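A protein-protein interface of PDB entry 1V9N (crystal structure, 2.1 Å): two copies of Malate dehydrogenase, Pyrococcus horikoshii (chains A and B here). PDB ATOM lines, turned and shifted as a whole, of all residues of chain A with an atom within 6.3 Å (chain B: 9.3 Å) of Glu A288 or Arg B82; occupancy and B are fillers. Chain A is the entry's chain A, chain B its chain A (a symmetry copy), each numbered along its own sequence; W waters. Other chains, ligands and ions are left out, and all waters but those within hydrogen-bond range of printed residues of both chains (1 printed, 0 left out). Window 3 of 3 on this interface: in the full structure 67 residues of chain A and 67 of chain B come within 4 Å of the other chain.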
ATOM      1  N   GLY A 142      31.540 -31.723 -17.982  1.00  0.00           N
ATOM      2  CA  GLY A 142      31.027 -30.364 -18.078  1.00  0.00           C
ATOM      3  C   GLY A 142      30.240 -30.098 -19.350  1.00  0.00           C
ATOM      4  O   GLY A 142      30.191 -28.966 -19.833  1.00  0.00           O
ATOM      5  N   ILE A 285      26.901 -31.887 -26.271  1.00  0.00           N
ATOM      6  CA  ILE A 285      26.890 -30.466 -26.544  1.00  0.00           C
ATOM      7  C   ILE A 285      27.854 -29.846 -25.547  1.00  0.00           C
ATOM      8  O   ILE A 285      27.670 -29.977 -24.337  1.00  0.00           O
ATOM      9  CB  ILE A 285      25.484 -29.855 -26.348  1.00  0.00           C
ATOM     10  CG1 ILE A 285      24.502 -30.449 -27.366  1.00  0.00           C
ATOM     11  CG2 ILE A 285      25.549 -28.339 -26.515  1.00  0.00           C
ATOM     12  CD1 ILE A 285      23.068 -29.924 -27.221  1.00  0.00           C
ATOM     13  N   ASP A 286      28.903 -29.200 -26.047  1.00  0.00           N
ATOM     14  CA  ASP A 286      29.861 -28.563 -25.151  1.00  0.00           C
ATOM     15  C   ASP A 286      29.255 -27.242 -24.700  1.00  0.00           C
ATOM     16  O   ASP A 286      29.294 -26.243 -25.414  1.00  0.00           O
ATOM     17  CB  ASP A 286      31.201 -28.317 -25.852  1.00  0.00           C
ATOM     18  CG  ASP A 286      32.222 -27.656 -24.935  1.00  0.00           C
ATOM     19  OD1 ASP A 286      32.369 -28.102 -23.776  1.00  0.00           O
ATOM     20  OD2 ASP A 286      32.886 -26.695 -25.371  1.00  0.00           O
ATOM     21  N   ILE A 287      28.676 -27.257 -23.509  1.00  0.00           N
ATOM     22  CA  ILE A 287      28.034 -26.077 -22.950  1.00  0.00           C
ATOM     23  C   ILE A 287      28.838 -24.783 -23.100  1.00  0.00           C
ATOM     24  O   ILE A 287      28.288 -23.758 -23.489  1.00  0.00           O
ATOM     25  CB  ILE A 287      27.708 -26.318 -21.462  1.00  0.00           C
ATOM     26  CG1 ILE A 287      26.651 -27.427 -21.352  1.00  0.00           C
ATOM     27  CG2 ILE A 287      27.215 -25.022 -20.805  1.00  0.00           C
ATOM     28  CD1 ILE A 287      26.482 -27.978 -19.943  1.00  0.00           C
ATOM     29  N   GLU A 288      30.134 -24.840 -22.805  1.00  0.00           N
ATOM     30  CA  GLU A 288      31.016 -23.667 -22.878  1.00  0.00           C
ATOM     31  C   GLU A 288      30.973 -22.919 -24.218  1.00  0.00           C
ATOM     32  O   GLU A 288      31.126 -21.699 -24.259  1.00  0.00           O
ATOM     33  CB  GLU A 288      32.458 -24.089 -22.557  1.00  0.00           C
ATOM     34  CG  GLU A 288      33.464 -22.944 -22.376  1.00  0.00           C
ATOM     35  CD  GLU A 288      33.222 -22.109 -21.125  1.00  0.00           C
ATOM     36  OE1 GLU A 288      32.438 -22.532 -20.246  1.00  0.00           O
ATOM     37  OE2 GLU A 288      33.830 -21.024 -21.013  1.00  0.00           O
ATOM     38  N   HIS A 289      30.777 -23.650 -25.313  1.00  0.00           N
ATOM     39  CA  HIS A 289      30.704 -23.036 -26.638  1.00  0.00           C
ATOM     40  C   HIS A 289      29.444 -22.178 -26.781  1.00  0.00           C
ATOM     41  O   HIS A 289      29.348 -21.352 -27.687  1.00  0.00           O
ATOM     42  CB  HIS A 289      30.693 -24.107 -27.736  1.00  0.00           C
ATOM     43  CG  HIS A 289      32.056 -24.567 -28.159  1.00  0.00           C
ATOM     44  ND1 HIS A 289      32.779 -25.509 -27.461  1.00  0.00           N
ATOM     45  CD2 HIS A 289      32.827 -24.210 -29.217  1.00  0.00           C
ATOM     46  CE1 HIS A 289      33.936 -25.715 -28.068  1.00  0.00           C
ATOM     47  NE2 HIS A 289      33.989 -24.938 -29.137  1.00  0.00           N
ATOM     48  N   PHE A 290      28.479 -22.385 -25.890  1.00  0.00           N
ATOM     49  CA  PHE A 290      27.226 -21.637 -25.926  1.00  0.00           C
ATOM     50  C   PHE A 290      27.183 -20.540 -24.871  1.00  0.00           C
ATOM     51  O   PHE A 290      27.010 -19.368 -25.199  1.00  0.00           O
ATOM     52  CB  PHE A 290      26.046 -22.593 -25.740  1.00  0.00           C
ATOM     53  CG  PHE A 290      25.770 -23.445 -26.941  1.00  0.00           C
ATOM     54  CD1 PHE A 290      24.768 -23.097 -27.840  1.00  0.00           C
ATOM     55  CD2 PHE A 290      26.525 -24.585 -27.187  1.00  0.00           C
ATOM     56  CE1 PHE A 290      24.519 -23.875 -28.965  1.00  0.00           C
ATOM     57  CE2 PHE A 290      26.285 -25.371 -28.315  1.00  0.00           C
ATOM     58  CZ  PHE A 290      25.278 -25.011 -29.204  1.00  0.00           C
ATOM     59  N   ILE A 291      27.321 -20.921 -23.605  1.00  0.00           N
ATOM     60  CA  ILE A 291      27.321 -19.950 -22.513  1.00  0.00           C
ATOM     61  C   ILE A 291      28.309 -20.418 -21.455  1.00  0.00           C
ATOM     62  O   ILE A 291      28.715 -21.577 -21.454  1.00  0.00           O
ATOM     63  CB  ILE A 291      25.919 -19.809 -21.863  1.00  0.00           C
ATOM     64  CG1 ILE A 291      25.492 -21.141 -21.239  1.00  0.00           C
ATOM     65  CG2 ILE A 291      24.901 -19.356 -22.912  1.00  0.00           C
ATOM     66  CD1 ILE A 291      24.266 -21.027 -20.351  1.00  0.00           C
ATOM     67  N   PRO A 292      28.726 -19.519 -20.546  1.00  0.00           N
ATOM     68  CA  PRO A 292      29.676 -19.969 -19.525  1.00  0.00           C
ATOM     69  C   PRO A 292      29.101 -21.145 -18.745  1.00  0.00           C
ATOM     70  O   PRO A 292      27.940 -21.112 -18.322  1.00  0.00           O
ATOM     71  CB  PRO A 292      29.871 -18.724 -18.664  1.00  0.00           C
ATOM     72  CG  PRO A 292      29.734 -17.604 -19.674  1.00  0.00           C
ATOM     73  CD  PRO A 292      28.532 -18.057 -20.485  1.00  0.00           C
ATOM     74  N   LEU A 293      29.906 -22.186 -18.562  1.00  0.00           N
ATOM     75  CA  LEU A 293      29.453 -23.368 -17.842  1.00  0.00           C
ATOM     76  C   LEU A 293      28.978 -23.026 -16.430  1.00  0.00           C
ATOM     77  O   LEU A 293      27.958 -23.541 -15.966  1.00  0.00           O
ATOM     78  CB  LEU A 293      30.573 -24.415 -17.778  1.00  0.00           C
ATOM     79  CG  LEU A 293      30.240 -25.669 -16.960  1.00  0.00           C
ATOM     80  CD1 LEU A 293      28.976 -26.315 -17.509  1.00  0.00           C
ATOM     81  CD2 LEU A 293      31.399 -26.645 -17.001  1.00  0.00           C
ATOM     82  N   GLU A 294      29.709 -22.155 -15.739  1.00  0.00           N
ATOM     83  CA  GLU A 294      29.305 -21.797 -14.386  1.00  0.00           C
ATOM     84  C   GLU A 294      27.940 -21.113 -14.374  1.00  0.00           C
ATOM     85  O   GLU A 294      27.179 -21.272 -13.424  1.00  0.00           O
ATOM     86  CB  GLU A 294      30.363 -20.916 -13.714  1.00  0.00           C
ATOM     87  CG  GLU A 294      31.635 -21.682 -13.311  1.00  0.00           C
ATOM     88  CD  GLU A 294      31.354 -22.890 -12.414  1.00  0.00           C
ATOM     89  OE1 GLU A 294      30.726 -22.714 -11.345  1.00  0.00           O
ATOM     90  OE2 GLU A 294      31.768 -24.018 -12.772  1.00  0.00           O
ATOM     91  N   ARG B  79      20.161 -11.803 -34.032  1.00  0.00           N
ATOM     92  CA  ARG B  79      21.615 -11.840 -33.946  1.00  0.00           C
ATOM     93  C   ARG B  79      22.265 -13.140 -33.481  1.00  0.00           C
ATOM     94  O   ARG B  79      21.781 -13.805 -32.565  1.00  0.00           O
ATOM     95  CB  ARG B  79      22.076 -10.698 -33.036  1.00  0.00           C
ATOM     96  CG  ARG B  79      23.556 -10.395 -33.102  1.00  0.00           C
ATOM     97  CD  ARG B  79      23.874  -9.090 -32.384  1.00  0.00           C
ATOM     98  NE  ARG B  79      23.874  -9.226 -30.929  1.00  0.00           N
ATOM     99  CZ  ARG B  79      24.793  -9.899 -30.243  1.00  0.00           C
ATOM    100  NH1 ARG B  79      25.789 -10.506 -30.878  1.00  0.00           N
ATOM    101  NH2 ARG B  79      24.721  -9.961 -28.918  1.00  0.00           N
ATOM    102  N   VAL B  80      23.381 -13.484 -34.118  1.00  0.00           N
ATOM    103  CA  VAL B  80      24.143 -14.677 -33.762  1.00  0.00           C
ATOM    104  C   VAL B  80      25.050 -14.297 -32.589  1.00  0.00           C
ATOM    105  O   VAL B  80      25.889 -13.408 -32.717  1.00  0.00           O
ATOM    106  CB  VAL B  80      25.014 -15.148 -34.938  1.00  0.00           C
ATOM    107  CG1 VAL B  80      25.856 -16.344 -34.515  1.00  0.00           C
ATOM    108  CG2 VAL B  80      24.130 -15.516 -36.124  1.00  0.00           C
ATOM    109  N   ILE B  81      24.861 -14.954 -31.449  1.00  0.00           N
ATOM    110  CA  ILE B  81      25.651 -14.683 -30.245  1.00  0.00           C
ATOM    111  C   ILE B  81      26.949 -15.497 -30.240  1.00  0.00           C
ATOM    112  O   ILE B  81      28.028 -14.962 -29.993  1.00  0.00           O
ATOM    113  CB  ILE B  81      24.855 -15.032 -28.967  1.00  0.00           C
ATOM    114  CG1 ILE B  81      23.516 -14.295 -28.965  1.00  0.00           C
ATOM    115  CG2 ILE B  81      25.660 -14.666 -27.735  1.00  0.00           C
ATOM    116  CD1 ILE B  81      23.634 -12.787 -29.022  1.00  0.00           C
ATOM    117  N   ARG B  82      26.825 -16.797 -30.488  1.00  0.00           N
ATOM    118  CA  ARG B  82      27.973 -17.702 -30.541  1.00  0.00           C
ATOM    119  C   ARG B  82      27.762 -18.546 -31.787  1.00  0.00           C
ATOM    120  O   ARG B  82      26.621 -18.809 -32.175  1.00  0.00           O
ATOM    121  CB  ARG B  82      28.027 -18.628 -29.310  1.00  0.00           C
ATOM    122  CG  ARG B  82      28.325 -17.944 -27.971  1.00  0.00           C
ATOM    123  CD  ARG B  82      29.686 -17.252 -27.970  1.00  0.00           C
ATOM    124  NE  ARG B  82      30.792 -18.185 -28.165  1.00  0.00           N
ATOM    125  CZ  ARG B  82      31.257 -19.007 -27.227  1.00  0.00           C
ATOM    126  NH1 ARG B  82      30.718 -19.016 -26.017  1.00  0.00           N
ATOM    127  NH2 ARG B  82      32.261 -19.826 -27.503  1.00  0.00           N
ATOM    128  N   GLU B  83      28.846 -18.982 -32.415  1.00  0.00           N
ATOM    129  CA  GLU B  83      28.700 -19.779 -33.617  1.00  0.00           C
ATOM    130  C   GLU B  83      29.917 -20.626 -33.941  1.00  0.00           C
ATOM    131  O   GLU B  83      31.048 -20.311 -33.550  1.00  0.00           O
ATOM    132  CB  GLU B  83      28.362 -18.864 -34.802  1.00  0.00           C
ATOM    133  CG  GLU B  83      28.325 -19.562 -36.159  1.00  0.00           C
ATOM    134  CD  GLU B  83      27.821 -18.658 -37.271  1.00  0.00           C
ATOM    135  OE1 GLU B  83      28.320 -17.520 -37.398  1.00  0.00           O
ATOM    136  OE2 GLU B  83      26.923 -19.090 -38.023  1.00  0.00           O
ATOM    137  N   GLY B  84      29.653 -21.722 -34.639  1.00  0.00           N
ATOM    138  CA  GLY B  84      30.691 -22.638 -35.061  1.00  0.00           C
ATOM    139  C   GLY B  84      30.223 -23.256 -36.368  1.00  0.00           C
ATOM    140  O   GLY B  84      29.095 -23.019 -36.786  1.00  0.00           O
ATOM    141  N   PRO B  85      31.064 -24.050 -37.042  1.00  0.00           N
ATOM    142  CA  PRO B  85      30.662 -24.668 -38.306  1.00  0.00           C
ATOM    143  C   PRO B  85      29.377 -25.498 -38.197  1.00  0.00           C
ATOM    144  O   PRO B  85      28.609 -25.598 -39.158  1.00  0.00           O
ATOM    145  CB  PRO B  85      31.878 -25.517 -38.668  1.00  0.00           C
ATOM    146  CG  PRO B  85      33.023 -24.689 -38.120  1.00  0.00           C
ATOM    147  CD  PRO B  85      32.489 -24.304 -36.758  1.00  0.00           C
ATOM    148  N   SER B  86      29.141 -26.082 -37.026  1.00  0.00           N
ATOM    149  CA  SER B  86      27.956 -26.913 -36.819  1.00  0.00           C
ATOM    150  C   SER B  86      26.949 -26.422 -35.779  1.00  0.00           C
ATOM    151  O   SER B  86      26.050 -27.170 -35.392  1.00  0.00           O
ATOM    152  CB  SER B  86      28.379 -28.344 -36.464  1.00  0.00           C
ATOM    153  OG  SER B  86      28.995 -28.977 -37.572  1.00  0.00           O
ATOM    154  N   TYR B  87      27.077 -25.181 -35.320  1.00  0.00           N
ATOM    155  CA  TYR B  87      26.124 -24.679 -34.332  1.00  0.00           C
ATOM    156  C   TYR B  87      26.053 -23.165 -34.287  1.00  0.00           C
ATOM    157  O   TYR B  87      26.913 -22.464 -34.831  1.00  0.00           O
ATOM    158  CB  TYR B  87      26.484 -25.193 -32.933  1.00  0.00           C
ATOM    159  CG  TYR B  87      27.539 -24.366 -32.227  1.00  0.00           C
ATOM    160  CD1 TYR B  87      27.184 -23.243 -31.478  1.00  0.00           C
ATOM    161  CD2 TYR B  87      28.897 -24.674 -32.349  1.00  0.00           C
ATOM    162  CE1 TYR B  87      28.154 -22.444 -30.871  1.00  0.00           C
ATOM    163  CE2 TYR B  87      29.871 -23.882 -31.748  1.00  0.00           C
ATOM    164  CZ  TYR B  87      29.491 -22.768 -31.010  1.00  0.00           C
ATOM    165  OH  TYR B  87      30.442 -21.987 -30.399  1.00  0.00           O
ATOM    166  N   ALA B  88      25.010 -22.670 -33.630  1.00  0.00           N
ATOM    167  CA  ALA B  88      24.821 -21.244 -33.449  1.00  0.00           C
ATOM    168  C   ALA B  88      23.845 -20.974 -32.305  1.00  0.00           C
ATOM    169  O   ALA B  88      22.916 -21.755 -32.053  1.00  0.00           O
ATOM    170  CB  ALA B  88      24.314 -20.606 -34.733  1.00  0.00           C
ATOM    171  N   LEU B  89      24.091 -19.883 -31.592  1.00  0.00           N
ATOM    172  CA  LEU B  89      23.222 -19.455 -30.507  1.00  0.00           C
ATOM    173  C   LEU B  89      22.656 -18.134 -31.021  1.00  0.00           C
ATOM    174  O   LEU B  89      23.394 -17.189 -31.286  1.00  0.00           O
ATOM    175  CB  LEU B  89      24.015 -19.256 -29.213  1.00  0.00           C
ATOM    176  CG  LEU B  89      23.289 -18.553 -28.061  1.00  0.00           C
ATOM    177  CD1 LEU B  89      21.948 -19.216 -27.795  1.00  0.00           C
ATOM    178  CD2 LEU B  89      24.169 -18.589 -26.816  1.00  0.00           C
ATOM    179  N   ILE B  90      21.340 -18.088 -31.173  1.00  0.00           N
ATOM    180  CA  ILE B  90      20.656 -16.921 -31.715  1.00  0.00           C
ATOM    181  C   ILE B  90      19.789 -16.187 -30.692  1.00  0.00           C
ATOM    182  O   ILE B  90      19.197 -16.809 -29.812  1.00  0.00           O
ATOM    183  CB  ILE B  90      19.705 -17.358 -32.869  1.00  0.00           C
ATOM    184  CG1 ILE B  90      20.486 -18.091 -33.966  1.00  0.00           C
ATOM    185  CG2 ILE B  90      18.930 -16.166 -33.397  1.00  0.00           C
ATOM    186  CD1 ILE B  90      21.594 -17.291 -34.602  1.00  0.00           C
ATOM    187  N   ASP B  91      19.719 -14.864 -30.818  1.00  0.00           N
ATOM    188  CA  ASP B  91      18.849 -14.066 -29.954  1.00  0.00           C
ATOM    189  C   ASP B  91      17.785 -13.516 -30.908  1.00  0.00           C
ATOM    190  O   ASP B  91      18.098 -12.776 -31.847  1.00  0.00           O
ATOM    191  CB  ASP B  91      19.603 -12.917 -29.278  1.00  0.00           C
ATOM    192  CG  ASP B  91      18.748 -12.198 -28.237  1.00  0.00           C
ATOM    193  OD1 ASP B  91      17.768 -11.533 -28.634  1.00  0.00           O
ATOM    194  OD2 ASP B  91      19.042 -12.311 -27.018  1.00  0.00           O
ATOM    195  N   LEU B 107      19.322 -21.799 -40.988  1.00  0.00           N
ATOM    196  CA  LEU B 107      20.747 -21.805 -40.659  1.00  0.00           C
ATOM    197  C   LEU B 107      21.212 -23.203 -40.251  1.00  0.00           C
ATOM    198  O   LEU B 107      22.311 -23.628 -40.612  1.00  0.00           O
ATOM    199  CB  LEU B 107      21.047 -20.810 -39.532  1.00  0.00           C
ATOM    200  CG  LEU B 107      22.503 -20.760 -39.057  1.00  0.00           C
ATOM    201  CD1 LEU B 107      23.406 -20.286 -40.200  1.00  0.00           C
ATOM    202  CD2 LEU B 107      22.616 -19.821 -37.863  1.00  0.00           C
ATOM    203  N   LYS B 111      24.170 -25.426 -42.110  1.00  0.00           N
ATOM    204  CA  LYS B 111      25.317 -25.989 -41.422  1.00  0.00           C
ATOM    205  C   LYS B 111      25.394 -27.508 -41.589  1.00  0.00           C
ATOM    206  O   LYS B 111      26.472 -28.056 -41.786  1.00  0.00           O
ATOM    207  CB  LYS B 111      25.280 -25.598 -39.942  1.00  0.00           C
ATOM    208  CG  LYS B 111      25.577 -24.103 -39.703  1.00  0.00           C
ATOM    209  CD  LYS B 111      25.595 -23.749 -38.222  1.00  0.00           C
ATOM    210  CE  LYS B 111      25.942 -22.274 -38.002  1.00  0.00           C
ATOM    211  NZ  LYS B 111      27.342 -21.942 -38.414  1.00  0.00           N
ATOM    212  N   ILE B 119      23.087 -27.515 -35.317  1.00  0.00           N
ATOM    213  CA  ILE B 119      22.311 -27.291 -34.100  1.00  0.00           C
ATOM    214  C   ILE B 119      22.205 -25.801 -33.823  1.00  0.00           C
ATOM    215  O   ILE B 119      23.203 -25.131 -33.557  1.00  0.00           O
ATOM    216  CB  ILE B 119      22.954 -27.993 -32.875  1.00  0.00           C
ATOM    217  CG1 ILE B 119      22.830 -29.511 -33.032  1.00  0.00           C
ATOM    218  CG2 ILE B 119      22.287 -27.522 -31.576  1.00  0.00           C
ATOM    219  CD1 ILE B 119      23.519 -30.313 -31.938  1.00  0.00           C
ATOM    220  N   VAL B 120      20.991 -25.276 -33.910  1.00  0.00           N
ATOM    221  CA  VAL B 120      20.785 -23.861 -33.655  1.00  0.00           C
ATOM    222  C   VAL B 120      19.801 -23.722 -32.510  1.00  0.00           C
ATOM    223  O   VAL B 120      18.745 -24.356 -32.498  1.00  0.00           O
ATOM    224  CB  VAL B 120      20.244 -23.119 -34.903  1.00  0.00           C
ATOM    225  CG1 VAL B 120      19.985 -21.656 -34.567  1.00  0.00           C
ATOM    226  CG2 VAL B 120      21.255 -23.211 -36.048  1.00  0.00           C
ATOM    227  N   ILE B 121      20.171 -22.909 -31.532  1.00  0.00           N
ATOM    228  CA  ILE B 121      19.320 -22.670 -30.385  1.00  0.00           C
ATOM    229  C   ILE B 121      19.015 -21.182 -30.320  1.00  0.00           C
ATOM    230  O   ILE B 121      19.880 -20.343 -30.584  1.00  0.00           O
ATOM    231  CB  ILE B 121      20.010 -23.155 -29.106  1.00  0.00           C
ATOM    232  CG1 ILE B 121      20.262 -24.665 -29.232  1.00  0.00           C
ATOM    233  CG2 ILE B 121      19.152 -22.855 -27.894  1.00  0.00           C
ATOM    234  CD1 ILE B 121      21.033 -25.268 -28.107  1.00  0.00           C
ATOM    235  N   ARG B 123      16.989 -17.857 -28.161  1.00  0.00           N
ATOM    236  CA  ARG B 123      16.379 -17.336 -26.946  1.00  0.00           C
ATOM    237  C   ARG B 123      15.758 -16.012 -27.351  1.00  0.00           C
ATOM    238  O   ARG B 123      15.934 -15.557 -28.487  1.00  0.00           O
ATOM    239  CB  ARG B 123      17.428 -17.089 -25.858  1.00  0.00           C
ATOM    240  CG  ARG B 123      18.368 -15.933 -26.173  1.00  0.00           C
ATOM    241  CD  ARG B 123      19.417 -15.764 -25.092  1.00  0.00           C
ATOM    242  NE  ARG B 123      20.301 -14.633 -25.369  1.00  0.00           N
ATOM    243  CZ  ARG B 123      21.588 -14.603 -25.039  1.00  0.00           C
ATOM    244  NH1 ARG B 123      22.132 -15.645 -24.427  1.00  0.00           N
ATOM    245  NH2 ARG B 123      22.326 -13.534 -25.309  1.00  0.00           N
ATOM    246  N   LEU B 259      20.381 -23.820 -21.836  1.00  0.00           N
ATOM    247  CA  LEU B 259      21.564 -23.793 -22.696  1.00  0.00           C
ATOM    248  C   LEU B 259      21.745 -22.505 -23.495  1.00  0.00           C
ATOM    249  O   LEU B 259      22.872 -22.102 -23.786  1.00  0.00           O
ATOM    250  CB  LEU B 259      21.527 -24.986 -23.655  1.00  0.00           C
ATOM    251  CG  LEU B 259      22.697 -25.158 -24.626  1.00  0.00           C
ATOM    252  CD1 LEU B 259      24.013 -25.321 -23.853  1.00  0.00           C
ATOM    253  CD2 LEU B 259      22.429 -26.378 -25.505  1.00  0.00           C
ATOM    254  N   SER B 260      20.642 -21.857 -23.851  1.00  0.00           N
ATOM    255  CA  SER B 260      20.705 -20.633 -24.638  1.00  0.00           C
ATOM    256  C   SER B 260      20.958 -19.379 -23.812  1.00  0.00           C
ATOM    257  O   SER B 260      21.214 -18.309 -24.364  1.00  0.00           O
ATOM    258  CB  SER B 260      19.396 -20.435 -25.396  1.00  0.00           C
ATOM    259  OG  SER B 260      18.354 -20.119 -24.485  1.00  0.00           O
HETATM  260  O   HOH W   1      31.230 -19.421 -22.814  1.00  0.00           O
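The backbone carbonyl oxygen of His A289 sits close to the guanidinium group of Arg B82.
O of Glu A288 is in hydrogen-bond range of NH1 of Arg B82 (3.2 Å).
O of His A289 lies within hydrogen-bond range of OH of Tyr B87.
O of Ala B88 lies within hydrogen-bond range of N of Ile B121, 3.0 Å away.
The side-chain carboxylate of Glu A288 lies within hydrogen-bond range of the backbone NH of Leu A293 (3.1 Å).
N of Ile B90 sits at hydrogen-bond distance from O of Ile B121 (2.8 Å).
ND1 of His A289 sits at hydrogen-bond distance from OD2 of Asp A286, at 2.4 Å.
The backbone carbonyl oxygen (O) of Leu B89 lies within hydrogen-bond range of the backbone NH (N) of Ile B81, 2.7 Å away.
The backbone NH (N) of Leu B89 lies within hydrogen-bond range of the backbone carbonyl oxygen (O) of Arg B82.
Leu B259 touches Ile A285.
CG of Arg B82 touches O of Phe A290 (3.4 Å).
Phe A290 touches Tyr B87.
Phe A290 touches Leu B89 (O to CD2, 3.4 Å).
Ile B121 touches Phe A290 (CD1 to CE1, 3.9 Å).
CB of Phe A290 touches O of Leu B259, at 3.8 Å.
Ile A291 touches Leu B259 (CG2 to O, 3.5 Å).
Glu A288 touches just one residue of chain B: Arg B82 (3.2 Å).
Of the printed residues of chain B, His A289 touches Arg B82 (3.1 Å) and Tyr B87 (3.0 Å).
Glu A294 touches none of the printed residues of chain B.
Arg B79 touches none of the printed residues of chain A.
Arg B82 touches just these residues of chain A: Glu A288 (3.2 Å), His A289 (3.1 Å) and Phe A290 (3.4 Å).
Of the printed residues of chain A, Leu B89 touches Phe A290.
Of the 11 printed residues of chain A, 5 touch a printed residue of chain B.
Hydrophobic or aromatic side chains of chain A within 4 Å of the printed part of chain B: Ile A285, His A289, Phe A290 and Ile A291.
Among the printed residues, no Asp or Glu carboxylate lies within 4 Å of a Lys or Arg side-chain nitrogen of the other chain.
No position is printed for both chains.
Of the 10 pairs that touch across the chains among the printed residues, none has its exchanged pair printed and touching as well.
Water W1 lies within hydrogen-bond range of the backbone carbonyl oxygen (O) of Glu A288 and the guanidinium group (NH1) of Arg B82.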
